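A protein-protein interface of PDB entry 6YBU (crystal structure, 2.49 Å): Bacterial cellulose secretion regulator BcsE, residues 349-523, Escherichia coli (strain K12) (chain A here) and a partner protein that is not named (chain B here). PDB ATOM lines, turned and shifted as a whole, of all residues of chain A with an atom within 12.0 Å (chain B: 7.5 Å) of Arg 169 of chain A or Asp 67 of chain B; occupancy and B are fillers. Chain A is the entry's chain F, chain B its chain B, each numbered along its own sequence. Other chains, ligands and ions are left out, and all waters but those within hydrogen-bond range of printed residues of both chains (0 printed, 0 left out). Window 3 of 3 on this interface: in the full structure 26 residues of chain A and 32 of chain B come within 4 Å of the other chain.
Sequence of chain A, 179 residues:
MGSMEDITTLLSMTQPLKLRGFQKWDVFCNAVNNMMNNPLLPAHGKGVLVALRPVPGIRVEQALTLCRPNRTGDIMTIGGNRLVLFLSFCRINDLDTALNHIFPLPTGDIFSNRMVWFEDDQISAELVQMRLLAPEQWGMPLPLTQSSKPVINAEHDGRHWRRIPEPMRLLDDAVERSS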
ATOM      1  N   PRO A 165       0.103   8.087  15.702  1.00  0.00           N
ATOM      2  CA  PRO A 165      -1.111   8.250  14.893  1.00  0.00           C
ATOM      3  C   PRO A 165      -1.756   6.905  14.595  1.00  0.00           C
ATOM      4  O   PRO A 165      -1.084   5.944  14.211  1.00  0.00           O
ATOM      5  CB  PRO A 165      -0.601   8.937  13.620  1.00  0.00           C
ATOM      6  CG  PRO A 165       0.863   8.628  13.578  1.00  0.00           C
ATOM      7  CD  PRO A 165       1.307   8.567  15.006  1.00  0.00           C
ATOM      8  N   GLU A 166      -3.073   6.841  14.780  1.00  0.00           N
ATOM      9  CA  GLU A 166      -3.818   5.605  14.596  1.00  0.00           C
ATOM     10  C   GLU A 166      -4.590   5.641  13.289  1.00  0.00           C
ATOM     11  O   GLU A 166      -5.243   6.651  12.989  1.00  0.00           O
ATOM     12  CB  GLU A 166      -4.789   5.383  15.761  1.00  0.00           C
ATOM     13  CG  GLU A 166      -4.113   5.099  17.086  1.00  0.00           C
ATOM     14  CD  GLU A 166      -5.111   4.885  18.207  1.00  0.00           C
ATOM     15  OE1 GLU A 166      -6.330   5.013  17.951  1.00  0.00           O
ATOM     16  OE2 GLU A 166      -4.679   4.589  19.342  1.00  0.00           O
ATOM     17  N   PRO A 167      -4.531   4.580  12.486  1.00  0.00           N
ATOM     18  CA  PRO A 167      -5.342   4.536  11.264  1.00  0.00           C
ATOM     19  C   PRO A 167      -6.826   4.663  11.579  1.00  0.00           C
ATOM     20  O   PRO A 167      -7.335   4.059  12.526  1.00  0.00           O
ATOM     21  CB  PRO A 167      -5.008   3.165  10.668  1.00  0.00           C
ATOM     22  CG  PRO A 167      -3.653   2.846  11.203  1.00  0.00           C
ATOM     23  CD  PRO A 167      -3.614   3.432  12.586  1.00  0.00           C
ATOM     24  N   MET A 168      -7.515   5.469  10.777  1.00  0.00           N
ATOM     25  CA  MET A 168      -8.943   5.678  10.941  1.00  0.00           C
ATOM     26  C   MET A 168      -9.570   5.840   9.564  1.00  0.00           C
ATOM     27  O   MET A 168      -8.879   6.007   8.557  1.00  0.00           O
ATOM     28  CB  MET A 168      -9.240   6.904  11.810  1.00  0.00           C
ATOM     29  CG  MET A 168      -8.885   8.222  11.146  1.00  0.00           C
ATOM     30  SD  MET A 168      -9.705   9.639  11.899  1.00  0.00           S
ATOM     31  CE  MET A 168     -11.418   9.273  11.526  1.00  0.00           C
ATOM     32  N   ARG A 169     -10.899   5.791   9.532  1.00  0.00           N
ATOM     33  CA  ARG A 169     -11.659   6.023   8.313  1.00  0.00           C
ATOM     34  C   ARG A 169     -12.458   7.309   8.466  1.00  0.00           C
ATOM     35  O   ARG A 169     -13.263   7.440   9.393  1.00  0.00           O
ATOM     36  CB  ARG A 169     -12.591   4.851   8.004  1.00  0.00           C
ATOM     37  CG  ARG A 169     -13.482   5.099   6.798  1.00  0.00           C
ATOM     38  CD  ARG A 169     -14.282   3.864   6.416  1.00  0.00           C
ATOM     39  NE  ARG A 169     -15.116   4.105   5.241  1.00  0.00           N
ATOM     40  CZ  ARG A 169     -14.679   4.031   3.988  1.00  0.00           C
ATOM     41  NH1 ARG A 169     -15.506   4.266   2.978  1.00  0.00           N
ATOM     42  NH2 ARG A 169     -13.413   3.723   3.742  1.00  0.00           N
ATOM     43  N   LEU A 170     -12.224   8.258   7.564  1.00  0.00           N
ATOM     44  CA  LEU A 170     -13.049   9.459   7.499  1.00  0.00           C
ATOM     45  C   LEU A 170     -14.421   9.075   6.959  1.00  0.00           C
ATOM     46  O   LEU A 170     -14.562   8.765   5.772  1.00  0.00           O
ATOM     47  CB  LEU A 170     -12.383  10.515   6.622  1.00  0.00           C
ATOM     48  CG  LEU A 170     -10.959  10.914   7.018  1.00  0.00           C
ATOM     49  CD1 LEU A 170     -10.411  11.986   6.088  1.00  0.00           C
ATOM     50  CD2 LEU A 170     -10.916  11.382   8.465  1.00  0.00           C
ATOM     51  N   LEU A 171     -15.427   9.080   7.831  1.00  0.00           N
ATOM     52  CA  LEU A 171     -16.746   8.588   7.465  1.00  0.00           C
ATOM     53  C   LEU A 171     -17.365   9.446   6.364  1.00  0.00           C
ATOM     54  O   LEU A 171     -17.006  10.611   6.162  1.00  0.00           O
ATOM     55  CB  LEU A 171     -17.663   8.554   8.687  1.00  0.00           C
ATOM     56  CG  LEU A 171     -17.300   7.528   9.764  1.00  0.00           C
ATOM     57  CD1 LEU A 171     -18.266   7.616  10.935  1.00  0.00           C
ATOM     58  CD2 LEU A 171     -17.284   6.121   9.184  1.00  0.00           C
ATOM     59  N   ASP A 172     -18.312   8.846   5.645  1.00  0.00           N
ATOM     60  CA  ASP A 172     -18.968   9.473   4.508  1.00  0.00           C
ATOM     61  C   ASP A 172     -20.476   9.430   4.698  1.00  0.00           C
ATOM     62  O   ASP A 172     -21.017   8.449   5.217  1.00  0.00           O
ATOM     63  CB  ASP A 172     -18.592   8.769   3.197  1.00  0.00           C
ATOM     64  CG  ASP A 172     -19.182   9.451   1.976  1.00  0.00           C
ATOM     65  OD1 ASP A 172     -19.608  10.618   2.087  1.00  0.00           O
ATOM     66  OD2 ASP A 172     -19.220   8.815   0.902  1.00  0.00           O
ATOM     67  N   ASP A 173     -21.147  10.496   4.272  1.00  0.00           N
ATOM     68  CA  ASP A 173     -22.606  10.544   4.281  1.00  0.00           C
ATOM     69  C   ASP A 173     -23.112  11.689   3.410  1.00  0.00           C
ATOM     70  O   ASP A 173     -23.175  12.836   3.852  1.00  0.00           O
ATOM     71  CB  ASP A 173     -23.141  10.693   5.706  1.00  0.00           C
ATOM     72  CG  ASP A 173     -24.595  10.284   5.825  1.00  0.00           C
ATOM     73  OD1 ASP A 173     -24.885   9.078   5.672  1.00  0.00           O
ATOM     74  OD2 ASP A 173     -25.447  11.164   6.067  1.00  0.00           O
ATOM     75  N   GLY B  57      -1.791   7.648   1.917  1.00  0.00           N
ATOM     76  CA  GLY B  57      -2.244   9.018   1.767  1.00  0.00           C
ATOM     77  C   GLY B  57      -3.423   9.057   0.825  1.00  0.00           C
ATOM     78  O   GLY B  57      -3.748   8.071   0.158  1.00  0.00           O
ATOM     79  N   TRP B  58      -4.069  10.225   0.775  1.00  0.00           N
ATOM     80  CA  TRP B  58      -5.286  10.339  -0.025  1.00  0.00           C
ATOM     81  C   TRP B  58      -4.984  10.259  -1.517  1.00  0.00           C
ATOM     82  O   TRP B  58      -5.724   9.614  -2.270  1.00  0.00           O
ATOM     83  CB  TRP B  58      -6.034  11.632   0.314  1.00  0.00           C
ATOM     84  CG  TRP B  58      -5.333  12.900  -0.077  1.00  0.00           C
ATOM     85  CD1 TRP B  58      -4.526  13.667   0.714  1.00  0.00           C
ATOM     86  CD2 TRP B  58      -5.394  13.561  -1.348  1.00  0.00           C
ATOM     87  NE1 TRP B  58      -4.073  14.757   0.012  1.00  0.00           N
ATOM     88  CE2 TRP B  58      -4.591  14.716  -1.257  1.00  0.00           C
ATOM     89  CE3 TRP B  58      -6.042  13.285  -2.557  1.00  0.00           C
ATOM     90  CZ2 TRP B  58      -4.421  15.595  -2.326  1.00  0.00           C
ATOM     91  CZ3 TRP B  58      -5.871  14.158  -3.618  1.00  0.00           C
ATOM     92  CH2 TRP B  58      -5.068  15.299  -3.495  1.00  0.00           C
ATOM     93  N   ALA B  61      -3.739   6.758  -2.434  1.00  0.00           N
ATOM     94  CA  ALA B  61      -4.844   5.807  -2.478  1.00  0.00           C
ATOM     95  C   ALA B  61      -5.647   5.944  -3.767  1.00  0.00           C
ATOM     96  O   ALA B  61      -6.136   4.945  -4.308  1.00  0.00           O
ATOM     97  CB  ALA B  61      -5.748   5.994  -1.260  1.00  0.00           C
ATOM     98  N   MET B  62      -5.797   7.170  -4.274  1.00  0.00           N
ATOM     99  CA  MET B  62      -6.562   7.367  -5.502  1.00  0.00           C
ATOM    100  C   MET B  62      -5.812   6.829  -6.714  1.00  0.00           C
ATOM    101  O   MET B  62      -6.420   6.246  -7.620  1.00  0.00           O
ATOM    102  CB  MET B  62      -6.887   8.849  -5.691  1.00  0.00           C
ATOM    103  CG  MET B  62      -7.858   9.412  -4.670  1.00  0.00           C
ATOM    104  SD  MET B  62      -8.253  11.139  -4.999  1.00  0.00           S
ATOM    105  CE  MET B  62      -9.150  11.564  -3.510  1.00  0.00           C
ATOM    106  N   ASP B  64      -3.831   4.336  -6.756  1.00  0.00           N
ATOM    107  CA  ASP B  64      -3.795   2.884  -6.667  1.00  0.00           C
ATOM    108  C   ASP B  64      -5.177   2.250  -6.718  1.00  0.00           C
ATOM    109  O   ASP B  64      -5.286   1.026  -6.604  1.00  0.00           O
ATOM    110  CB  ASP B  64      -3.076   2.455  -5.383  1.00  0.00           C
ATOM    111  CG  ASP B  64      -1.638   2.932  -5.332  1.00  0.00           C
ATOM    112  OD1 ASP B  64      -1.150   3.462  -6.353  1.00  0.00           O
ATOM    113  OD2 ASP B  64      -0.997   2.781  -4.270  1.00  0.00           O
ATOM    114  N   GLY B  65      -6.232   3.048  -6.882  1.00  0.00           N
ATOM    115  CA  GLY B  65      -7.583   2.535  -6.946  1.00  0.00           C
ATOM    116  C   GLY B  65      -8.248   2.285  -5.610  1.00  0.00           C
ATOM    117  O   GLY B  65      -9.374   1.772  -5.587  1.00  0.00           O
ATOM    118  N   GLN B  66      -7.601   2.637  -4.501  1.00  0.00           N
ATOM    119  CA  GLN B  66      -8.137   2.371  -3.177  1.00  0.00           C
ATOM    120  C   GLN B  66      -8.966   3.557  -2.683  1.00  0.00           C
ATOM    121  O   GLN B  66      -9.073   4.596  -3.339  1.00  0.00           O
ATOM    122  CB  GLN B  66      -7.005   2.045  -2.205  1.00  0.00           C
ATOM    123  CG  GLN B  66      -6.215   0.802  -2.575  1.00  0.00           C
ATOM    124  CD  GLN B  66      -5.201   0.417  -1.517  1.00  0.00           C
ATOM    125  OE1 GLN B  66      -5.040  -0.760  -1.197  1.00  0.00           O
ATOM    126  NE2 GLN B  66      -4.510   1.410  -0.969  1.00  0.00           N
ATOM    127  N   ASP B  67      -9.558   3.398  -1.504  1.00  0.00           N
ATOM    128  CA  ASP B  67     -10.420   4.419  -0.921  1.00  0.00           C
ATOM    129  C   ASP B  67      -9.580   5.362  -0.065  1.00  0.00           C
ATOM    130  O   ASP B  67      -8.983   4.938   0.933  1.00  0.00           O
ATOM    131  CB  ASP B  67     -11.531   3.775  -0.093  1.00  0.00           C
ATOM    132  CG  ASP B  67     -12.634   4.751   0.269  1.00  0.00           C
ATOM    133  OD1 ASP B  67     -12.529   5.940  -0.101  1.00  0.00           O
ATOM    134  OD2 ASP B  67     -13.614   4.327   0.919  1.00  0.00           O
ATOM    135  N   TRP B  68      -9.544   6.640  -0.453  1.00  0.00           N
ATOM    136  CA  TRP B  68      -8.755   7.628   0.273  1.00  0.00           C
ATOM    137  C   TRP B  68      -9.250   7.839   1.695  1.00  0.00           C
ATOM    138  O   TRP B  68      -8.483   8.305   2.544  1.00  0.00           O
ATOM    139  CB  TRP B  68      -8.765   8.960  -0.479  1.00  0.00           C
ATOM    140  CG  TRP B  68     -10.139   9.537  -0.650  1.00  0.00           C
ATOM    141  CD1 TRP B  68     -10.984   9.336  -1.700  1.00  0.00           C
ATOM    142  CD2 TRP B  68     -10.829  10.405   0.259  1.00  0.00           C
ATOM    143  NE1 TRP B  68     -12.155  10.025  -1.505  1.00  0.00           N
ATOM    144  CE2 TRP B  68     -12.086  10.689  -0.310  1.00  0.00           C
ATOM    145  CE3 TRP B  68     -10.505  10.969   1.498  1.00  0.00           C
ATOM    146  CZ2 TRP B  68     -13.020  11.512   0.316  1.00  0.00           C
ATOM    147  CZ3 TRP B  68     -11.434  11.787   2.118  1.00  0.00           C
ATOM    148  CH2 TRP B  68     -12.675  12.051   1.525  1.00  0.00           C
ATOM    149  N   ARG B  69     -10.514   7.513   1.976  1.00  0.00           N
ATOM    150  CA  ARG B  69     -11.051   7.702   3.318  1.00  0.00           C
ATOM    151  C   ARG B  69     -10.376   6.801   4.344  1.00  0.00           C
ATOM    152  O   ARG B  69     -10.371   7.134   5.534  1.00  0.00           O
ATOM    153  CB  ARG B  69     -12.563   7.464   3.311  1.00  0.00           C
ATOM    154  CG  ARG B  69     -13.311   8.370   2.346  1.00  0.00           C
ATOM    155  CD  ARG B  69     -14.813   8.149   2.396  1.00  0.00           C
ATOM    156  NE  ARG B  69     -15.505   8.981   1.416  1.00  0.00           N
ATOM    157  CZ  ARG B  69     -15.954  10.209   1.657  1.00  0.00           C
ATOM    158  NH1 ARG B  69     -15.791  10.751   2.857  1.00  0.00           N
ATOM    159  NH2 ARG B  69     -16.572  10.893   0.703  1.00  0.00           N
ATOM    160  N   ASP B  70      -9.798   5.680   3.915  1.00  0.00           N
ATOM    161  CA  ASP B  70      -9.056   4.802   4.810  1.00  0.00           C
ATOM    162  C   ASP B  70      -7.632   5.280   5.063  1.00  0.00           C
ATOM    163  O   ASP B  70      -6.901   4.622   5.811  1.00  0.00           O
ATOM    164  CB  ASP B  70      -9.025   3.379   4.246  1.00  0.00           C
ATOM    165  CG  ASP B  70     -10.402   2.749   4.178  1.00  0.00           C
ATOM    166  OD1 ASP B  70     -11.260   3.105   5.014  1.00  0.00           O
ATOM    167  OD2 ASP B  70     -10.626   1.898   3.291  1.00  0.00           O
ATOM    168  N   ALA B  71      -7.222   6.398   4.467  1.00  0.00           N
ATOM    169  CA  ALA B  71      -5.878   6.930   4.646  1.00  0.00           C
ATOM    170  C   ALA B  71      -5.793   7.957   5.768  1.00  0.00           C
ATOM    171  O   ALA B  71      -4.743   8.590   5.933  1.00  0.00           O
ATOM    172  CB  ALA B  71      -5.380   7.547   3.337  1.00  0.00           C
ATOM    173  N   GLY B  72      -6.864   8.136   6.540  1.00  0.00           N
ATOM    174  CA  GLY B  72      -6.832   9.080   7.635  1.00  0.00           C
ATOM    175  C   GLY B  72      -6.031   8.568   8.815  1.00  0.00           C
ATOM    176  O   GLY B  72      -5.779   7.374   8.970  1.00  0.00           O
ATOM    177  N   LEU B  73      -5.620   9.507   9.666  1.00  0.00           N
ATOM    178  CA  LEU B  73      -4.826   9.192  10.847  1.00  0.00           C
ATOM    179  C   LEU B  73      -5.268  10.081  11.998  1.00  0.00           C
ATOM    180  O   LEU B  73      -5.308  11.307  11.859  1.00  0.00           O
ATOM    181  CB  LEU B  73      -3.329   9.382  10.575  1.00  0.00           C
ATOM    182  CG  LEU B  73      -2.678   8.405   9.595  1.00  0.00           C
ATOM    183  CD1 LEU B  73      -1.258   8.838   9.272  1.00  0.00           C
ATOM    184  CD2 LEU B  73      -2.694   6.995  10.158  1.00  0.00           C
ATOM    185  N   ARG B  74      -5.595   9.461  13.130  1.00  0.00           N
ATOM    186  CA  ARG B  74      -6.000  10.188  14.325  1.00  0.00           C
ATOM    187  C   ARG B  74      -4.767  10.485  15.169  1.00  0.00           C
ATOM    188  O   ARG B  74      -4.055   9.562  15.579  1.00  0.00           O
ATOM    189  CB  ARG B  74      -7.019   9.382  15.128  1.00  0.00           C
ATOM    190  CG  ARG B  74      -7.547  10.099  16.358  1.00  0.00           C
ATOM    191  CD  ARG B  74      -8.596   9.263  17.079  1.00  0.00           C
ATOM    192  NE  ARG B  74      -9.615   8.763  16.161  1.00  0.00           N
ATOM    193  CZ  ARG B  74     -10.656   9.473  15.739  1.00  0.00           C
ATOM    194  NH1 ARG B  74     -10.819  10.724  16.151  1.00  0.00           N
ATOM    195  NH2 ARG B  74     -11.532   8.933  14.900  1.00  0.00           N
ATOM    196  N   ASP B  80      -7.280  15.154  13.477  1.00  0.00           N
ATOM    197  CA  ASP B  80      -7.098  14.081  12.509  1.00  0.00           C
ATOM    198  C   ASP B  80      -6.223  14.568  11.361  1.00  0.00           C
ATOM    199  O   ASP B  80      -6.245  15.748  10.997  1.00  0.00           O
ATOM    200  CB  ASP B  80      -8.442  13.585  11.964  1.00  0.00           C
ATOM    201  CG  ASP B  80      -9.271  12.877  13.014  1.00  0.00           C
ATOM    202  OD1 ASP B  80      -8.691  12.405  14.016  1.00  0.00           O
ATOM    203  OD2 ASP B  80     -10.505  12.789  12.834  1.00  0.00           O
ATOM    204  N   TYR B 118     -15.834  18.468  11.848  1.00  0.00           N
ATOM    205  CA  TYR B 118     -14.699  19.305  12.205  1.00  0.00           C
ATOM    206  C   TYR B 118     -15.103  20.772  12.206  1.00  0.00           C
ATOM    207  O   TYR B 118     -15.840  21.224  11.322  1.00  0.00           O
ATOM    208  CB  TYR B 118     -13.535  19.100  11.231  1.00  0.00           C
ATOM    209  CG  TYR B 118     -13.142  17.655  11.038  1.00  0.00           C
ATOM    210  CD1 TYR B 118     -12.277  17.027  11.927  1.00  0.00           C
ATOM    211  CD2 TYR B 118     -13.630  16.920   9.965  1.00  0.00           C
ATOM    212  CE1 TYR B 118     -11.912  15.706  11.753  1.00  0.00           C
ATOM    213  CE2 TYR B 118     -13.271  15.600   9.782  1.00  0.00           C
ATOM    214  CZ  TYR B 118     -12.413  14.996  10.680  1.00  0.00           C
ATOM    215  OH  TYR B 118     -12.055  13.681  10.501  1.00  0.00           O
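Of the 9 printed residues of chain A, 8 touch a printed residue of chain B.
Printed residues of chain A that touch a printed residue of chain B: Pro 165, Glu 166, Pro 167, Met 168, Arg 169, Leu 170, Leu 171 and Asp 172.
Hydrophobic or aromatic side chains of chain A within 4 Å of the printed part of chain B: Met 168 and Leu 170.
Along chain A the printed residues that touch a printed residue of chain B span positions 165 to 172.
OD1 of Asp 80 of chain B lies within salt-bridge range of NH1 of Arg 74 of chain B.
The side-chain carboxylate (OD1) of Asp 67 of chain B sits close to the backbone NH (N) of Arg 69 of chain B, at 3.3 Å.
OH of Tyr 118 of chain B lies within hydrogen-bond range of OD2 of Asp 80 of chain B, at 2.9 Å.
Of chain B, only Asp 67 (2.8 Å), Arg 69 (3.3 Å) and Asp 70 (2.6 Å) come within 4 Å of Arg 169 of chain A.
Asp 67 of chain B touches just one residue of chain A: Arg 169.
Gly 57 of chain B touches none of the printed residues of chain A.
No residue of chain A comes within 4 Å of Ala 61 of chain B.
No residue of chain A comes within 4 Å of Met 62 of chain B.
No residue of chain A comes within 4 Å of Gly 65 of chain B.
No residue of chain A comes within 4 Å of Gln 66 of chain B.
No residue of chain A comes within 4 Å of Trp 68 of chain B.
Of chain A, only Met 168 (3.6 Å), Arg 169 (3.3 Å), Leu 170 (3.0 Å), Leu 171 (3.5 Å) and Asp 172 (3.2 Å) come within 4 Å of Arg 69 of chain B.
Of chain A, only Met 168 and Arg 169 come within 4 Å of Asp 70 of chain B.
No residue of chain A comes within 4 Å of Ala 71 of chain B.
Of the printed residues of chain A, Leu 73 of chain B touches Glu 166, Pro 167 and Met 168.
Printed residues of chain B within 4 Å of Glu 166 of chain A: Leu 73 and Arg 74.
Of the printed residues of chain B, Leu 171 of chain A touches Arg 69.
Printed residues of chain B within 4 Å of Leu 170 of chain A: Arg 69 and Tyr 118.
Asp 64 of chain B touches none of the printed residues of chain A.
The nearest residue of chain B that does not touch Arg 169 of chain A is Gly 72 of chain B (5.4 Å).
The nearest residue of chain A that does not touch Asp 67 of chain B is Leu 170 of chain A (6.6 Å).
Among the printed residues, pairs that only touch across the chains: Arg 169 of chain A with Arg 69 of chain B (3.3 Å), Leu 170 of chain A with Tyr 118 of chain B (3.3 Å), Pro 165 of chain A with Arg 74 of chain B (3.3 Å), Glu 166 of chain A with Leu 73 of chain B (3.3 Å), Leu 171 of chain A with Arg 69 of chain B (3.5 Å), Met 168 of chain A with Arg 69 of chain B (3.6 Å), Met 168 of chain A with Asp 70 of chain B (3.7 Å), Pro 167 of chain A with Gly 72 of chain B (3.7 Å), Pro 167 of chain A with Leu 73 of chain B (3.8 Å) and Met 168 of chain A with Leu 73 of chain B (3.8 Å).
NH2 of Arg 74 of chain B sits close to SD of Met 168 of chain A (3.6 Å).
The backbone NH of Arg 74 of chain B is in hydrogen-bond range of the backbone carbonyl oxygen of Glu 166 of chain A (2.8 Å).
The side-chain carboxylate (OD1) of Asp 172 of chain A lies within salt-bridge range of the guanidinium group (NH2) of Arg 69 of chain B (3.3 Å).
OD1 of Asp 70 of chain B is in salt-bridge range of NH2 of Arg 169 of chain A (2.6 Å).
The side-chain carboxylate of Asp 67 of chain B lies within salt-bridge range of the guanidinium group of Arg 169 of chain A.
N of Leu 170 of chain A lies within hydrogen-bond range of O of Arg 69 of chain B, 3.0 Å away.
The side-chain carboxylate (OD2) of Asp 80 of chain B sits close to the side-chain sulfur (SD) of Met 168 of chain A.
The backbone NH of Met 168 of chain A sits at hydrogen-bond distance from the backbone carbonyl oxygen of Gly 72 of chain B.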
